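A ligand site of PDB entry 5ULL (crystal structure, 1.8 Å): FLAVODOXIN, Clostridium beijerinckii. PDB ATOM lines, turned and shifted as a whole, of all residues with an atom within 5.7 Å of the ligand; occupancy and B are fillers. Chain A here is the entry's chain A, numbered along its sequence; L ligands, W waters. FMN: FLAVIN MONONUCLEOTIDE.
OG of Ser 7 is in hydrogen-bond range of O3P of the ligand, at 2.7 Å. OE2 of Glu 59 is in hydrogen-bond range of N3 of the ligand, at 3.0 Å. N of Trp 90 is in hydrogen-bond range of O2 of the ligand, at 3.0 Å. The backbone NH (N) of Gly 91 lies within hydrogen-bond range of an oxygen (O2) of the ligand (2.7 Å). N of Gly 10 is in hydrogen-bond range of O2P of the ligand, at 3.1 Å. O3P of the ligand is in hydrogen-bond range of N of Thr 12 (2.7 Å). N of Glu 59 is in hydrogen-bond range of O4 of the ligand (2.8 Å). O4' of the ligand sits at hydrogen-bond distance from OG of Ser 87. OG1 of Thr 9 sits at hydrogen-bond distance from O2P of the ligand (2.6 Å). N of Ala 55 sits at hydrogen-bond distance from O2' of the ligand, at 3.3 Å. An oxygen (O2P) of the ligand is in hydrogen-bond range of the backbone NH of Asn 11 (3.0 Å). An oxygen (O3P) of the ligand lies within hydrogen-bond range of the side-chain hydroxyl (OG1) of Thr 12, 2.9 Å away. An oxygen (O1P) of the ligand sits at hydrogen-bond distance from the backbone NH (N) of Gly 8 (2.8 Å). The backbone carbonyl oxygen (O) of Ala 55 sits at hydrogen-bond distance from an oxygen (O2') of the ligand (2.7 Å). N of Gly 89 is in hydrogen-bond range of N1 of the ligand (3.0 Å). The backbone NH (N) of Thr 9 sits at hydrogen-bond distance from an oxygen (O2P) of the ligand (2.8 Å). The side-chain amide oxygen of Asn 11 sits at hydrogen-bond distance from an oxygen (O4') of the ligand (2.8 Å). O1P of the ligand is in hydrogen-bond range of OG of Ser 54, at 2.8 Å.
The backbone NH of Trp 95 lies within hydrogen-bond range of the side-chain carboxylate of Glu 59, at 3.0 Å. The backbone NH (N) of Asn 119 lies within hydrogen-bond range of the backbone carbonyl oxygen (O) of Tyr 88 (2.8 Å). The side-chain hydroxyl of Ser 7 lies within hydrogen-bond range of the backbone NH of Asn 11. O of Ser 87 lies within hydrogen-bond range of N of Ala 55. The side-chain hydroxyl (OG) of Ser 7 sits at hydrogen-bond distance from the backbone NH (N) of Thr 12. The side-chain hydroxyl (OG) of Ser 7 lies within hydrogen-bond range of the backbone NH (N) of Gly 10, at 3.0 Å. OG of Ser 7 is in hydrogen-bond range of N of Glu 13. N of Ser 87 sits at hydrogen-bond distance from OG1 of Thr 12.
The backbone carbonyl oxygen (O) of Gly 57 lies close to a nitrogen (N5) of the ligand (3.0 Å). Trp 6 touches the ligand (CZ3 to O1P, 3.9 Å). Met 56 touches the ligand. Asp 58 touches the ligand (C to O4, 3.8 Å). Tyr 88 touches the ligand. CA of Asn 119 touches O4' of the ligand (3.5 Å). Hydrophobic or aromatic side chains within 4 Å of the ligand: Trp 6, Ala 55, Met 56, Tyr 88 and Trp 90. Of the 26 residues printed, 19 come within 4 Å of the ligand. The nearest printed residue that does not touch the ligand is Glu 13 (4.4 Å).
Water W5 bridges the side-chain amide oxygen (OD1) of Asn 119 and an oxygen (O3') of the ligand. Water W2 lies within hydrogen-bond range of an oxygen (O4) of the ligand, the side-chain carboxylate of Asp 58 and the indole nitrogen of Trp 90. Water W1 bridges O1P of the ligand (2.7 Å) and SD of Met 56 (3.7 Å). Water W4 lies within hydrogen-bond range of the side-chain carboxylate (OE1) of Glu 59 (2.8 Å), an oxygen (O2) of the ligand (3.2 Å) and the backbone NH (N) of Asp 92 (3.5 Å). Water W6 lies within hydrogen-bond range of the side-chain sulfur of Met 56 (2.5 Å), the backbone carbonyl oxygen of Ala 55 (2.7 Å), the side-chain hydroxyl of Ser 54 (2.7 Å) and an oxygen (O2') of the ligand (3.3 Å).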
ATOM      1  N   TRP A   6     -36.076 -30.851 -14.361  1.00  0.00           N
ATOM      2  CA  TRP A   6     -35.450 -31.192 -15.637  1.00  0.00           C
ATOM      3  C   TRP A   6     -33.981 -31.283 -15.254  1.00  0.00           C
ATOM      4  O   TRP A   6     -33.480 -30.416 -14.539  1.00  0.00           O
ATOM      5  CB  TRP A   6     -35.631 -30.123 -16.718  1.00  0.00           C
ATOM      6  CG  TRP A   6     -34.992 -30.568 -18.030  1.00  0.00           C
ATOM      7  CD1 TRP A   6     -35.564 -31.330 -18.995  1.00  0.00           C
ATOM      8  CD2 TRP A   6     -33.621 -30.367 -18.439  1.00  0.00           C
ATOM      9  NE1 TRP A   6     -34.637 -31.665 -19.962  1.00  0.00           N
ATOM     10  CE2 TRP A   6     -33.435 -31.081 -19.645  1.00  0.00           C
ATOM     11  CE3 TRP A   6     -32.529 -29.671 -17.886  1.00  0.00           C
ATOM     12  CZ2 TRP A   6     -32.207 -31.123 -20.316  1.00  0.00           C
ATOM     13  CZ3 TRP A   6     -31.300 -29.713 -18.558  1.00  0.00           C
ATOM     14  CH2 TRP A   6     -31.155 -30.434 -19.766  1.00  0.00           C
ATOM     15  N   SER A   7     -33.308 -32.340 -15.700  1.00  0.00           N
ATOM     16  CA  SER A   7     -31.890 -32.523 -15.409  1.00  0.00           C
ATOM     17  C   SER A   7     -31.193 -33.121 -16.634  1.00  0.00           C
ATOM     18  O   SER A   7     -31.638 -34.145 -17.162  1.00  0.00           O
ATOM     19  CB  SER A   7     -31.738 -33.420 -14.203  1.00  0.00           C
ATOM     20  OG  SER A   7     -30.377 -33.529 -13.807  1.00  0.00           O
ATOM     21  N   GLY A   8     -30.111 -32.488 -17.081  1.00  0.00           N
ATOM     22  CA  GLY A   8     -29.383 -32.974 -18.245  1.00  0.00           C
ATOM     23  C   GLY A   8     -28.323 -34.006 -17.962  1.00  0.00           C
ATOM     24  O   GLY A   8     -28.058 -34.858 -18.799  1.00  0.00           O
ATOM     25  N   THR A   9     -27.655 -33.911 -16.811  1.00  0.00           N
ATOM     26  CA  THR A   9     -26.613 -34.878 -16.461  1.00  0.00           C
ATOM     27  C   THR A   9     -26.886 -35.585 -15.132  1.00  0.00           C
ATOM     28  O   THR A   9     -26.120 -36.482 -14.741  1.00  0.00           O
ATOM     29  CB  THR A   9     -25.179 -34.261 -16.466  1.00  0.00           C
ATOM     30  OG1 THR A   9     -24.992 -33.444 -15.312  1.00  0.00           O
ATOM     31  CG2 THR A   9     -24.959 -33.428 -17.704  1.00  0.00           C
ATOM     32  N   GLY A  10     -27.967 -35.216 -14.466  1.00  0.00           N
ATOM     33  CA  GLY A  10     -28.305 -35.840 -13.196  1.00  0.00           C
ATOM     34  C   GLY A  10     -28.062 -34.992 -11.966  1.00  0.00           C
ATOM     35  O   GLY A  10     -28.453 -35.378 -10.861  1.00  0.00           O
ATOM     36  N   ASN A  11     -27.489 -33.808 -12.114  1.00  0.00           N
ATOM     37  CA  ASN A  11     -27.221 -32.971 -10.942  1.00  0.00           C
ATOM     38  C   ASN A  11     -28.478 -32.463 -10.267  1.00  0.00           C
ATOM     39  O   ASN A  11     -28.659 -32.642  -9.056  1.00  0.00           O
ATOM     40  CB  ASN A  11     -26.256 -31.831 -11.276  1.00  0.00           C
ATOM     41  CG  ASN A  11     -24.896 -32.323 -11.681  1.00  0.00           C
ATOM     42  OD1 ASN A  11     -24.130 -31.623 -12.335  1.00  0.00           O
ATOM     43  ND2 ASN A  11     -24.565 -33.538 -11.288  1.00  0.00           N
ATOM     44  N   THR A  12     -29.373 -31.848 -11.043  1.00  0.00           N
ATOM     45  CA  THR A  12     -30.626 -31.350 -10.486  1.00  0.00           C
ATOM     46  C   THR A  12     -31.512 -32.536 -10.070  1.00  0.00           C
ATOM     47  O   THR A  12     -32.278 -32.428  -9.099  1.00  0.00           O
ATOM     48  CB  THR A  12     -31.379 -30.446 -11.495  1.00  0.00           C
ATOM     49  OG1 THR A  12     -30.519 -29.365 -11.869  1.00  0.00           O
ATOM     50  CG2 THR A  12     -32.654 -29.870 -10.876  1.00  0.00           C
ATOM     51  N   GLU A  13     -31.363 -33.665 -10.756  1.00  0.00           N
ATOM     52  CA  GLU A  13     -32.129 -34.870 -10.415  1.00  0.00           C
ATOM     53  C   GLU A  13     -31.755 -35.330  -9.010  1.00  0.00           C
ATOM     54  O   GLU A  13     -32.620 -35.712  -8.217  1.00  0.00           O
ATOM     55  CB  GLU A  13     -31.844 -35.998 -11.420  1.00  0.00           C
ATOM     56  CG  GLU A  13     -32.661 -37.283 -11.143  1.00  0.00           C
ATOM     57  CD  GLU A  13     -32.461 -38.390 -12.183  1.00  0.00           C
ATOM     58  OE1 GLU A  13     -31.592 -38.257 -13.070  1.00  0.00           O
ATOM     59  OE2 GLU A  13     -33.165 -39.418 -12.111  1.00  0.00           O
ATOM     60  N   SER A  54     -31.685 -26.907 -14.014  1.00  0.00           N
ATOM     61  CA  SER A  54     -30.324 -26.372 -14.021  1.00  0.00           C
ATOM     62  C   SER A  54     -30.234 -25.151 -14.924  1.00  0.00           C
ATOM     63  O   SER A  54     -31.150 -24.874 -15.712  1.00  0.00           O
ATOM     64  CB  SER A  54     -29.354 -27.441 -14.546  1.00  0.00           C
ATOM     65  OG  SER A  54     -29.840 -27.987 -15.759  1.00  0.00           O
ATOM     66  N   ALA A  55     -29.115 -24.432 -14.807  1.00  0.00           N
ATOM     67  CA  ALA A  55     -28.876 -23.256 -15.648  1.00  0.00           C
ATOM     68  C   ALA A  55     -28.507 -23.762 -17.044  1.00  0.00           C
ATOM     69  O   ALA A  55     -27.680 -24.665 -17.178  1.00  0.00           O
ATOM     70  CB  ALA A  55     -27.766 -22.423 -15.066  1.00  0.00           C
ATOM     71  N   MET A  56     -29.177 -23.235 -18.078  1.00  0.00           N
ATOM     72  CA  MET A  56     -28.930 -23.646 -19.466  1.00  0.00           C
ATOM     73  C   MET A  56     -28.748 -22.442 -20.414  1.00  0.00           C
ATOM     74  O   MET A  56     -28.930 -21.285 -20.010  1.00  0.00           O
ATOM     75  CB  MET A  56     -30.052 -24.546 -19.983  1.00  0.00           C
ATOM     76  CG  MET A  56     -30.076 -25.934 -19.360  1.00  0.00           C
ATOM     77  SD  MET A  56     -28.650 -26.953 -19.838  1.00  0.00           S
ATOM     78  CE  MET A  56     -28.980 -27.086 -21.561  1.00  0.00           C
ATOM     79  N   GLY A  57     -28.377 -22.725 -21.660  1.00  0.00           N
ATOM     80  CA  GLY A  57     -28.143 -21.678 -22.633  1.00  0.00           C
ATOM     81  C   GLY A  57     -27.213 -20.669 -22.003  1.00  0.00           C
ATOM     82  O   GLY A  57     -26.129 -21.011 -21.526  1.00  0.00           O
ATOM     83  N   ASP A  58     -27.630 -19.402 -22.002  1.00  0.00           N
ATOM     84  CA  ASP A  58     -26.853 -18.358 -21.347  1.00  0.00           C
ATOM     85  C   ASP A  58     -27.752 -17.830 -20.251  1.00  0.00           C
ATOM     86  O   ASP A  58     -28.566 -16.916 -20.464  1.00  0.00           O
ATOM     87  CB  ASP A  58     -26.461 -17.242 -22.325  1.00  0.00           C
ATOM     88  CG  ASP A  58     -25.587 -16.174 -21.677  1.00  0.00           C
ATOM     89  OD1 ASP A  58     -24.903 -16.459 -20.646  1.00  0.00           O
ATOM     90  OD2 ASP A  58     -25.568 -15.033 -22.189  1.00  0.00           O
ATOM     91  N   GLU A  59     -27.666 -18.492 -19.095  1.00  0.00           N
ATOM     92  CA  GLU A  59     -28.438 -18.158 -17.893  1.00  0.00           C
ATOM     93  C   GLU A  59     -29.938 -18.161 -18.116  1.00  0.00           C
ATOM     94  O   GLU A  59     -30.630 -17.195 -17.747  1.00  0.00           O
ATOM     95  CB  GLU A  59     -27.968 -16.841 -17.282  1.00  0.00           C
ATOM     96  CG  GLU A  59     -26.502 -16.843 -16.827  1.00  0.00           C
ATOM     97  CD  GLU A  59     -26.205 -17.680 -15.592  1.00  0.00           C
ATOM     98  OE1 GLU A  59     -27.121 -18.119 -14.887  1.00  0.00           O
ATOM     99  OE2 GLU A  59     -25.011 -17.895 -15.307  1.00  0.00           O
ATOM    100  N   VAL A  60     -30.454 -19.230 -18.698  1.00  0.00           N
ATOM    101  CA  VAL A  60     -31.887 -19.368 -18.941  1.00  0.00           C
ATOM    102  C   VAL A  60     -32.384 -20.762 -18.510  1.00  0.00           C
ATOM    103  O   VAL A  60     -31.571 -21.623 -18.151  1.00  0.00           O
ATOM    104  CB  VAL A  60     -32.249 -19.152 -20.441  1.00  0.00           C
ATOM    105  CG1 VAL A  60     -31.962 -17.716 -20.861  1.00  0.00           C
ATOM    106  CG2 VAL A  60     -31.486 -20.120 -21.336  1.00  0.00           C
ATOM    107  N   SER A  87     -29.269 -26.793 -10.147  1.00  0.00           N
ATOM    108  CA  SER A  87     -27.820 -26.879 -10.137  1.00  0.00           C
ATOM    109  C   SER A  87     -27.290 -25.935 -11.215  1.00  0.00           C
ATOM    110  O   SER A  87     -27.960 -25.683 -12.219  1.00  0.00           O
ATOM    111  CB  SER A  87     -27.391 -28.325 -10.442  1.00  0.00           C
ATOM    112  OG  SER A  87     -25.985 -28.460 -10.396  1.00  0.00           O
ATOM    113  N   TYR A  88     -26.099 -25.379 -11.008  1.00  0.00           N
ATOM    114  CA  TYR A  88     -25.528 -24.496 -12.012  1.00  0.00           C
ATOM    115  C   TYR A  88     -24.048 -24.780 -12.094  1.00  0.00           C
ATOM    116  O   TYR A  88     -23.500 -25.508 -11.256  1.00  0.00           O
ATOM    117  CB  TYR A  88     -25.811 -23.030 -11.684  1.00  0.00           C
ATOM    118  CG  TYR A  88     -25.162 -22.552 -10.423  1.00  0.00           C
ATOM    119  CD1 TYR A  88     -25.674 -22.911  -9.171  1.00  0.00           C
ATOM    120  CD2 TYR A  88     -24.022 -21.741 -10.465  1.00  0.00           C
ATOM    121  CE1 TYR A  88     -25.067 -22.479  -7.996  1.00  0.00           C
ATOM    122  CE2 TYR A  88     -23.408 -21.303  -9.300  1.00  0.00           C
ATOM    123  CZ  TYR A  88     -23.931 -21.675  -8.073  1.00  0.00           C
ATOM    124  OH  TYR A  88     -23.339 -21.238  -6.914  1.00  0.00           O
ATOM    125  N   GLY A  89     -23.386 -24.215 -13.100  1.00  0.00           N
ATOM    126  CA  GLY A  89     -21.976 -24.492 -13.273  1.00  0.00           C
ATOM    127  C   GLY A  89     -20.989 -23.373 -13.129  1.00  0.00           C
ATOM    128  O   GLY A  89     -20.231 -23.335 -12.174  1.00  0.00           O
ATOM    129  N   TRP A  90     -21.001 -22.434 -14.055  1.00  0.00           N
ATOM    130  CA  TRP A  90     -20.033 -21.346 -14.019  1.00  0.00           C
ATOM    131  C   TRP A  90     -20.510 -19.963 -13.604  1.00  0.00           C
ATOM    132  O   TRP A  90     -19.688 -19.099 -13.307  1.00  0.00           O
ATOM    133  CB  TRP A  90     -19.321 -21.262 -15.366  1.00  0.00           C
ATOM    134  CG  TRP A  90     -20.256 -21.216 -16.549  1.00  0.00           C
ATOM    135  CD1 TRP A  90     -20.931 -20.122 -17.006  1.00  0.00           C
ATOM    136  CD2 TRP A  90     -20.603 -22.303 -17.423  1.00  0.00           C
ATOM    137  NE1 TRP A  90     -21.680 -20.458 -18.111  1.00  0.00           N
ATOM    138  CE2 TRP A  90     -21.490 -21.787 -18.388  1.00  0.00           C
ATOM    139  CE3 TRP A  90     -20.244 -23.657 -17.478  1.00  0.00           C
ATOM    140  CZ2 TRP A  90     -22.040 -22.586 -19.408  1.00  0.00           C
ATOM    141  CZ3 TRP A  90     -20.785 -24.444 -18.496  1.00  0.00           C
ATOM    142  CH2 TRP A  90     -21.676 -23.906 -19.439  1.00  0.00           C
ATOM    143  N   GLY A  91     -21.825 -19.740 -13.583  1.00  0.00           N
ATOM    144  CA  GLY A  91     -22.340 -18.434 -13.212  1.00  0.00           C
ATOM    145  C   GLY A  91     -22.513 -18.289 -11.710  1.00  0.00           C
ATOM    146  O   GLY A  91     -21.905 -19.048 -10.946  1.00  0.00           O
ATOM    147  N   ASP A  92     -23.313 -17.316 -11.285  1.00  0.00           N
ATOM    148  CA  ASP A  92     -23.584 -17.103  -9.873  1.00  0.00           C
ATOM    149  C   ASP A  92     -25.063 -17.065  -9.512  1.00  0.00           C
ATOM    150  O   ASP A  92     -25.455 -16.480  -8.504  1.00  0.00           O
ATOM    151  CB  ASP A  92     -22.858 -15.866  -9.313  1.00  0.00           C
ATOM    152  CG  ASP A  92     -23.273 -14.555  -9.989  1.00  0.00           C
ATOM    153  OD1 ASP A  92     -24.383 -14.460 -10.552  1.00  0.00           O
ATOM    154  OD2 ASP A  92     -22.475 -13.600  -9.939  1.00  0.00           O
ATOM    155  N   TRP A  95     -29.754 -17.186 -13.697  1.00  0.00           N
ATOM    156  CA  TRP A  95     -30.945 -17.850 -14.219  1.00  0.00           C
ATOM    157  C   TRP A  95     -32.021 -18.058 -13.124  1.00  0.00           C
ATOM    158  O   TRP A  95     -33.212 -18.000 -13.409  1.00  0.00           O
ATOM    159  CB  TRP A  95     -30.569 -19.193 -14.925  1.00  0.00           C
ATOM    160  CG  TRP A  95     -30.838 -20.435 -14.125  1.00  0.00           C
ATOM    161  CD1 TRP A  95     -31.834 -21.348 -14.348  1.00  0.00           C
ATOM    162  CD2 TRP A  95     -30.135 -20.893 -12.959  1.00  0.00           C
ATOM    163  NE1 TRP A  95     -31.804 -22.332 -13.390  1.00  0.00           N
ATOM    164  CE2 TRP A  95     -30.765 -22.079 -12.526  1.00  0.00           C
ATOM    165  CE3 TRP A  95     -29.026 -20.412 -12.233  1.00  0.00           C
ATOM    166  CZ2 TRP A  95     -30.340 -22.796 -11.390  1.00  0.00           C
ATOM    167  CZ3 TRP A  95     -28.594 -21.123 -11.107  1.00  0.00           C
ATOM    168  CH2 TRP A  95     -29.258 -22.315 -10.700  1.00  0.00           C
ATOM    169  N   VAL A 117     -27.190 -25.056  -6.139  1.00  0.00           N
ATOM    170  CA  VAL A 117     -25.966 -25.793  -5.812  1.00  0.00           C
ATOM    171  C   VAL A 117     -25.108 -25.897  -7.055  1.00  0.00           C
ATOM    172  O   VAL A 117     -25.622 -26.068  -8.169  1.00  0.00           O
ATOM    173  CB  VAL A 117     -26.294 -27.225  -5.323  1.00  0.00           C
ATOM    174  CG1 VAL A 117     -25.027 -28.050  -5.146  1.00  0.00           C
ATOM    175  CG2 VAL A 117     -27.068 -27.151  -4.004  1.00  0.00           C
ATOM    176  N   GLN A 118     -23.804 -25.747  -6.871  1.00  0.00           N
ATOM    177  CA  GLN A 118     -22.891 -25.829  -7.997  1.00  0.00           C
ATOM    178  C   GLN A 118     -22.550 -27.273  -8.321  1.00  0.00           C
ATOM    179  O   GLN A 118     -22.068 -28.021  -7.471  1.00  0.00           O
ATOM    180  CB  GLN A 118     -21.622 -25.030  -7.721  1.00  0.00           C
ATOM    181  CG  GLN A 118     -20.778 -24.832  -8.967  1.00  0.00           C
ATOM    182  CD  GLN A 118     -19.477 -24.113  -8.700  1.00  0.00           C
ATOM    183  OE1 GLN A 118     -19.178 -23.757  -7.548  1.00  0.00           O
ATOM    184  NE2 GLN A 118     -18.690 -23.889  -9.740  1.00  0.00           N
ATOM    185  N   ASN A 119     -22.832 -27.662  -9.559  1.00  0.00           N
ATOM    186  CA  ASN A 119     -22.564 -29.019 -10.050  1.00  0.00           C
ATOM    187  C   ASN A 119     -23.281 -30.059  -9.183  1.00  0.00           C
ATOM    188  O   ASN A 119     -24.386 -29.799  -8.724  1.00  0.00           O
ATOM    189  CB  ASN A 119     -21.041 -29.249 -10.156  1.00  0.00           C
ATOM    190  CG  ASN A 119     -20.352 -28.194 -11.042  1.00  0.00           C
ATOM    191  OD1 ASN A 119     -20.664 -28.055 -12.241  1.00  0.00           O
ATOM    192  ND2 ASN A 119     -19.468 -27.413 -10.450  1.00  0.00           N
ATOM    193  N   GLU A 120     -22.675 -31.215  -8.933  1.00  0.00           N
ATOM    194  CA  GLU A 120     -23.341 -32.242  -8.120  1.00  0.00           C
ATOM    195  C   GLU A 120     -23.379 -31.880  -6.633  1.00  0.00           C
ATOM    196  O   GLU A 120     -22.391 -31.410  -6.079  1.00  0.00           O
ATOM    197  CB  GLU A 120     -22.670 -33.610  -8.293  1.00  0.00           C
ATOM    198  CG  GLU A 120     -23.417 -34.760  -7.610  1.00  0.00           C
ATOM    199  CD  GLU A 120     -22.638 -36.074  -7.544  1.00  0.00           C
ATOM    200  OE1 GLU A 120     -21.380 -36.038  -7.518  1.00  0.00           O
ATOM    201  OE2 GLU A 120     -23.281 -37.145  -7.496  1.00  0.00           O
HETATM  202  N1  FMN L   1     -24.184 -22.996 -15.748  1.00  0.00           N
HETATM  203  C2  FMN L   1     -24.233 -21.708 -15.327  1.00  0.00           C
HETATM  204  O2  FMN L   1     -23.847 -21.403 -14.243  1.00  0.00           O
HETATM  205  N3  FMN L   1     -24.751 -20.714 -16.163  1.00  0.00           N
HETATM  206  C4  FMN L   1     -25.163 -20.938 -17.452  1.00  0.00           C
HETATM  207  O4  FMN L   1     -25.515 -20.019 -18.176  1.00  0.00           O
HETATM  208  C4A FMN L   1     -25.100 -22.372 -17.916  1.00  0.00           C
HETATM  209  N5  FMN L   1     -25.403 -22.693 -19.165  1.00  0.00           N
HETATM  210  C5A FMN L   1     -25.181 -24.002 -19.588  1.00  0.00           C
HETATM  211  C6  FMN L   1     -25.388 -24.358 -20.958  1.00  0.00           C
HETATM  212  C7  FMN L   1     -25.260 -25.665 -21.376  1.00  0.00           C
HETATM  213  C7M FMN L   1     -25.481 -26.050 -22.810  1.00  0.00           C
HETATM  214  C8  FMN L   1     -24.888 -26.667 -20.422  1.00  0.00           C
HETATM  215  C8M FMN L   1     -24.801 -28.139 -20.798  1.00  0.00           C
HETATM  216  C9  FMN L   1     -24.632 -26.330 -19.109  1.00  0.00           C
HETATM  217  C9A FMN L   1     -24.771 -25.011 -18.671  1.00  0.00           C
HETATM  218  N10 FMN L   1     -24.462 -24.645 -17.372  1.00  0.00           N
HETATM  219  C10 FMN L   1     -24.587 -23.341 -16.944  1.00  0.00           C
HETATM  220  C1' FMN L   1     -23.952 -25.663 -16.442  1.00  0.00           C
HETATM  221  C2' FMN L   1     -25.063 -26.533 -15.817  1.00  0.00           C
HETATM  222  O2' FMN L   1     -26.088 -25.721 -15.250  1.00  0.00           O
HETATM  223  C3' FMN L   1     -24.460 -27.418 -14.724  1.00  0.00           C
HETATM  224  O3' FMN L   1     -23.484 -28.281 -15.299  1.00  0.00           O
HETATM  225  C4' FMN L   1     -25.451 -28.240 -13.866  1.00  0.00           C
HETATM  226  O4' FMN L   1     -24.732 -28.943 -12.842  1.00  0.00           O
HETATM  227  C5' FMN L   1     -26.276 -29.167 -14.738  1.00  0.00           C
HETATM  228  O5' FMN L   1     -27.246 -29.844 -13.938  1.00  0.00           O
HETATM  229  P   FMN L   1     -28.004 -30.982 -14.649  1.00  0.00           P
HETATM  230  O1P FMN L   1     -28.503 -30.494 -15.928  1.00  0.00           O
HETATM  231  O2P FMN L   1     -27.244 -32.256 -14.628  1.00  0.00           O
HETATM  232  O3P FMN L   1     -29.150 -31.184 -13.643  1.00  0.00           O
HETATM  233  O   HOH W   1     -27.085 -29.924 -18.214  1.00  0.00           O
HETATM  234  O   HOH W   2     -23.535 -18.518 -19.267  1.00  0.00           O
HETATM  235  O   HOH W   3     -24.408 -29.795 -17.601  1.00  0.00           O
HETATM  236  O   HOH W   4     -25.759 -19.298 -12.710  1.00  0.00           O
HETATM  237  O   HOH W   5     -21.694 -29.623 -14.008  1.00  0.00           O
HETATM  238  O   HOH W   6     -27.843 -27.308 -17.480  1.00  0.00           O
